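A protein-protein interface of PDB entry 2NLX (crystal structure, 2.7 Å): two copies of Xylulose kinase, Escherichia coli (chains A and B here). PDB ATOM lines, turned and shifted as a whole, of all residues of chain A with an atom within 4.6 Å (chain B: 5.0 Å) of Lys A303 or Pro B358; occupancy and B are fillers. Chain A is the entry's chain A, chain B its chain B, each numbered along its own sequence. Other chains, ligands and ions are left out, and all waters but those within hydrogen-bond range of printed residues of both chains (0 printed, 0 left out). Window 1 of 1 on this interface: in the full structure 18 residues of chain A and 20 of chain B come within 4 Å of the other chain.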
ATOM      1  N   ASP A 299     -19.633  15.404  16.861  1.00  0.00           N
ATOM      2  CA  ASP A 299     -18.334  15.764  16.340  1.00  0.00           C
ATOM      3  C   ASP A 299     -18.208  17.247  16.108  1.00  0.00           C
ATOM      4  O   ASP A 299     -17.206  17.854  16.433  1.00  0.00           O
ATOM      5  CB  ASP A 299     -18.074  15.028  15.039  1.00  0.00           C
ATOM      6  CG  ASP A 299     -17.469  13.685  15.257  1.00  0.00           C
ATOM      7  OD1 ASP A 299     -17.479  12.871  14.324  1.00  0.00           O
ATOM      8  OD2 ASP A 299     -16.967  13.341  16.334  1.00  0.00           O
ATOM      9  N   TRP A 300     -19.233  17.820  15.509  1.00  0.00           N
ATOM     10  CA  TRP A 300     -19.186  19.199  15.093  1.00  0.00           C
ATOM     11  C   TRP A 300     -19.046  20.071  16.320  1.00  0.00           C
ATOM     12  O   TRP A 300     -18.316  21.047  16.320  1.00  0.00           O
ATOM     13  CB  TRP A 300     -20.451  19.543  14.307  1.00  0.00           C
ATOM     14  CG  TRP A 300     -20.790  20.981  14.326  1.00  0.00           C
ATOM     15  CD1 TRP A 300     -20.296  21.937  13.520  1.00  0.00           C
ATOM     16  CD2 TRP A 300     -21.701  21.631  15.208  1.00  0.00           C
ATOM     17  NE1 TRP A 300     -20.834  23.154  13.843  1.00  0.00           N
ATOM     18  CE2 TRP A 300     -21.703  22.985  14.881  1.00  0.00           C
ATOM     19  CE3 TRP A 300     -22.515  21.197  16.252  1.00  0.00           C
ATOM     20  CZ2 TRP A 300     -22.486  23.905  15.547  1.00  0.00           C
ATOM     21  CZ3 TRP A 300     -23.280  22.103  16.912  1.00  0.00           C
ATOM     22  CH2 TRP A 300     -23.269  23.441  16.561  1.00  0.00           C
ATOM     23  N   ALA A 301     -19.737  19.676  17.381  1.00  0.00           N
ATOM     24  CA  ALA A 301     -19.812  20.436  18.615  1.00  0.00           C
ATOM     25  C   ALA A 301     -18.560  20.269  19.427  1.00  0.00           C
ATOM     26  O   ALA A 301     -18.168  21.147  20.167  1.00  0.00           O
ATOM     27  CB  ALA A 301     -20.972  19.983  19.403  1.00  0.00           C
ATOM     28  N   ALA A 302     -17.936  19.117  19.294  1.00  0.00           N
ATOM     29  CA  ALA A 302     -16.709  18.866  19.999  1.00  0.00           C
ATOM     30  C   ALA A 302     -15.585  19.706  19.441  1.00  0.00           C
ATOM     31  O   ALA A 302     -14.606  19.978  20.112  1.00  0.00           O
ATOM     32  CB  ALA A 302     -16.371  17.423  19.941  1.00  0.00           C
ATOM     33  N   LYS A 303     -15.734  20.143  18.212  1.00  0.00           N
ATOM     34  CA  LYS A 303     -14.713  20.963  17.621  1.00  0.00           C
ATOM     35  C   LYS A 303     -15.006  22.443  17.765  1.00  0.00           C
ATOM     36  O   LYS A 303     -14.115  23.237  18.014  1.00  0.00           O
ATOM     37  CB  LYS A 303     -14.510  20.609  16.161  1.00  0.00           C
ATOM     38  CG  LYS A 303     -13.279  21.235  15.581  1.00  0.00           C
ATOM     39  CD  LYS A 303     -12.646  22.176  16.600  1.00  0.00           C
ATOM     40  CE  LYS A 303     -11.157  22.348  16.373  1.00  0.00           C
ATOM     41  NZ  LYS A 303     -10.874  23.181  15.179  1.00  0.00           N
ATOM     42  N   LEU A 304     -16.263  22.812  17.610  1.00  0.00           N
ATOM     43  CA  LEU A 304     -16.662  24.184  17.796  1.00  0.00           C
ATOM     44  C   LEU A 304     -16.139  24.654  19.119  1.00  0.00           C
ATOM     45  O   LEU A 304     -15.916  25.829  19.320  1.00  0.00           O
ATOM     46  CB  LEU A 304     -18.170  24.289  17.785  1.00  0.00           C
ATOM     47  CG  LEU A 304     -18.718  25.666  17.497  1.00  0.00           C
ATOM     48  CD1 LEU A 304     -18.559  25.962  16.045  1.00  0.00           C
ATOM     49  CD2 LEU A 304     -20.154  25.698  17.898  1.00  0.00           C
ATOM     50  N   THR A 305     -15.947  23.705  20.026  1.00  0.00           N
ATOM     51  CA  THR A 305     -15.699  24.008  21.413  1.00  0.00           C
ATOM     52  C   THR A 305     -14.245  23.848  21.723  1.00  0.00           C
ATOM     53  O   THR A 305     -13.787  24.259  22.773  1.00  0.00           O
ATOM     54  CB  THR A 305     -16.488  23.084  22.300  1.00  0.00           C
ATOM     55  OG1 THR A 305     -16.665  21.834  21.648  1.00  0.00           O
ATOM     56  CG2 THR A 305     -17.876  23.579  22.458  1.00  0.00           C
ATOM     57  N   GLY A 306     -13.519  23.218  20.817  1.00  0.00           N
ATOM     58  CA  GLY A 306     -12.099  23.032  20.986  1.00  0.00           C
ATOM     59  C   GLY A 306     -11.759  21.816  21.806  1.00  0.00           C
ATOM     60  O   GLY A 306     -10.708  21.750  22.425  1.00  0.00           O
ATOM     61  N   THR B 305     -14.947  29.014  22.288  1.00  0.00           N
ATOM     62  CA  THR B 305     -14.338  28.132  21.305  1.00  0.00           C
ATOM     63  C   THR B 305     -12.982  27.627  21.780  1.00  0.00           C
ATOM     64  O   THR B 305     -12.065  27.463  20.982  1.00  0.00           O
ATOM     65  CB  THR B 305     -14.159  28.842  19.955  1.00  0.00           C
ATOM     66  OG1 THR B 305     -13.290  29.969  20.121  1.00  0.00           O
ATOM     67  CG2 THR B 305     -15.506  29.305  19.415  1.00  0.00           C
ATOM     68  N   HIS B 356     -20.598  24.679  11.052  1.00  0.00           N
ATOM     69  CA  HIS B 356     -19.154  24.651  10.884  1.00  0.00           C
ATOM     70  C   HIS B 356     -18.529  25.545  11.922  1.00  0.00           C
ATOM     71  O   HIS B 356     -19.217  26.075  12.779  1.00  0.00           O
ATOM     72  CB  HIS B 356     -18.720  25.427   9.662  1.00  0.00           C
ATOM     73  CG  HIS B 356     -19.046  24.723   8.390  1.00  0.00           C
ATOM     74  ND1 HIS B 356     -19.437  23.404   8.366  1.00  0.00           N
ATOM     75  CD2 HIS B 356     -19.062  25.146   7.108  1.00  0.00           C
ATOM     76  CE1 HIS B 356     -19.680  23.045   7.123  1.00  0.00           C
ATOM     77  NE2 HIS B 356     -19.465  24.084   6.339  1.00  0.00           N
ATOM     78  N   GLY B 357     -17.215  25.680  11.865  1.00  0.00           N
ATOM     79  CA  GLY B 357     -16.021  25.497  12.658  1.00  0.00           C
ATOM     80  C   GLY B 357     -15.833  26.608  13.655  1.00  0.00           C
ATOM     81  O   GLY B 357     -16.683  27.453  13.802  1.00  0.00           O
ATOM     82  N   PRO B 358     -14.707  26.604  14.339  1.00  0.00           N
ATOM     83  CA  PRO B 358     -14.466  27.522  15.440  1.00  0.00           C
ATOM     84  C   PRO B 358     -13.915  28.867  14.992  1.00  0.00           C
ATOM     85  O   PRO B 358     -14.389  29.901  15.438  1.00  0.00           O
ATOM     86  CB  PRO B 358     -13.423  26.782  16.265  1.00  0.00           C
ATOM     87  CG  PRO B 358     -13.071  25.624  15.460  1.00  0.00           C
ATOM     88  CD  PRO B 358     -14.259  25.254  14.672  1.00  0.00           C
ATOM     89  N   ASN B 359     -12.911  28.850  14.129  1.00  0.00           N
ATOM     90  CA  ASN B 359     -12.506  30.059  13.447  1.00  0.00           C
ATOM     91  C   ASN B 359     -13.560  30.592  12.481  1.00  0.00           C
ATOM     92  O   ASN B 359     -13.414  31.692  11.953  1.00  0.00           O
ATOM     93  CB  ASN B 359     -11.166  29.838  12.732  1.00  0.00           C
ATOM     94  CG  ASN B 359     -11.118  28.547  11.924  1.00  0.00           C
ATOM     95  OD1 ASN B 359     -10.169  28.327  11.170  1.00  0.00           O
ATOM     96  ND2 ASN B 359     -12.126  27.685  12.084  1.00  0.00           N
ATOM     97  N   GLU B 360     -14.625  29.825  12.257  1.00  0.00           N
ATOM     98  CA  GLU B 360     -15.709  30.259  11.365  1.00  0.00           C
ATOM     99  C   GLU B 360     -16.703  31.006  12.252  1.00  0.00           C
ATOM    100  O   GLU B 360     -17.402  31.926  11.816  1.00  0.00           O
ATOM    101  CB  GLU B 360     -16.437  29.059  10.733  1.00  0.00           C
ATOM    102  CG  GLU B 360     -15.622  27.775  10.657  1.00  0.00           C
ATOM    103  CD  GLU B 360     -14.653  27.791   9.516  1.00  0.00           C
ATOM    104  OE1 GLU B 360     -13.547  27.225   9.659  1.00  0.00           O
ATOM    105  OE2 GLU B 360     -15.006  28.370   8.469  1.00  0.00           O
ATOM    106  N   LEU B 361     -16.763  30.570  13.506  1.00  0.00           N
ATOM    107  CA  LEU B 361     -17.647  31.158  14.492  1.00  0.00           C
ATOM    108  C   LEU B 361     -16.957  32.412  15.021  1.00  0.00           C
ATOM    109  O   LEU B 361     -17.618  33.379  15.400  1.00  0.00           O
ATOM    110  CB  LEU B 361     -17.905  30.148  15.621  1.00  0.00           C
ATOM    111  CG  LEU B 361     -18.875  30.522  16.746  1.00  0.00           C
ATOM    112  CD1 LEU B 361     -20.273  30.744  16.181  1.00  0.00           C
ATOM    113  CD2 LEU B 361     -18.891  29.418  17.787  1.00  0.00           C
ATOM    114  N   ALA B 362     -15.624  32.383  15.034  1.00  0.00           N
ATOM    115  CA  ALA B 362     -14.828  33.520  15.489  1.00  0.00           C
ATOM    116  C   ALA B 362     -15.081  34.673  14.524  1.00  0.00           C
ATOM    117  O   ALA B 362     -15.060  35.842  14.909  1.00  0.00           O
ATOM    118  CB  ALA B 362     -13.351  33.163  15.502  1.00  0.00           C
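Lys A303 touches Pro B358 (NZ to CG, 3.3 Å).
Thr B305 touches Leu A304 (CA to O, 3.4 Å).
Leu A304 touches His B356.
CD1 of Leu A304 touches O of Gly B357, at 3.3 Å.
Leu B361 touches Leu A304.
Thr A305 touches Thr B305.
The backbone carbonyl oxygen of Ala A302 is in hydrogen-bond range of the side-chain hydroxyl of Thr A305, 3.2 Å away.
The backbone NH (N) of His B356 lies close to the indole nitrogen (NE1) of Trp A300.
Thr B305 touches its own counterpart, Thr A305.
1 position is printed for both chains.
Of the 7 pairs that touch across the chains among the printed residues, 1 has its exchanged pair printed and touching as well.
Of the 8 printed residues of chain A, 4 touch a printed residue of chain B.
Hydrophobic or aromatic side chains of chain A that line the printed part of chain B: Trp A300 and Leu A304.
Of the 8 printed residues of chain B, 5 touch a printed residue of chain A.
Printed residues of chain B that touch a printed residue of chain A: Thr B305, His B356, Gly B357, Pro B358 and Leu B361.
Of the printed residues of chain B, Trp A300 touches His B356.
Of chain B, only Pro B358 (3.3 Å) comes within 4 Å of Lys A303.
Of the printed residues of chain B, Thr A305 touches Thr B305.
Of the printed residues of chain A, Thr B305 touches Leu A304 (3.4 Å) and Thr A305 (3.6 Å).
Printed residues of chain A within 4 Å of His B356: Trp A300 (3.2 Å) and Leu A304 (3.3 Å).
Of the printed residues of chain A, Gly B357 touches Leu A304 (3.3 Å).
Of chain A, only Lys A303 comes within 4 Å of Pro B358.
The nearest printed residue of chain B that does not touch Lys A303 is Thr B305 (5.6 Å).
The nearest residue of chain A that does not touch Pro B358 is Leu A304 (4.1 Å).
The nearest printed residue of chain B that does not touch Trp A300 is Gly B357 (4.8 Å).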
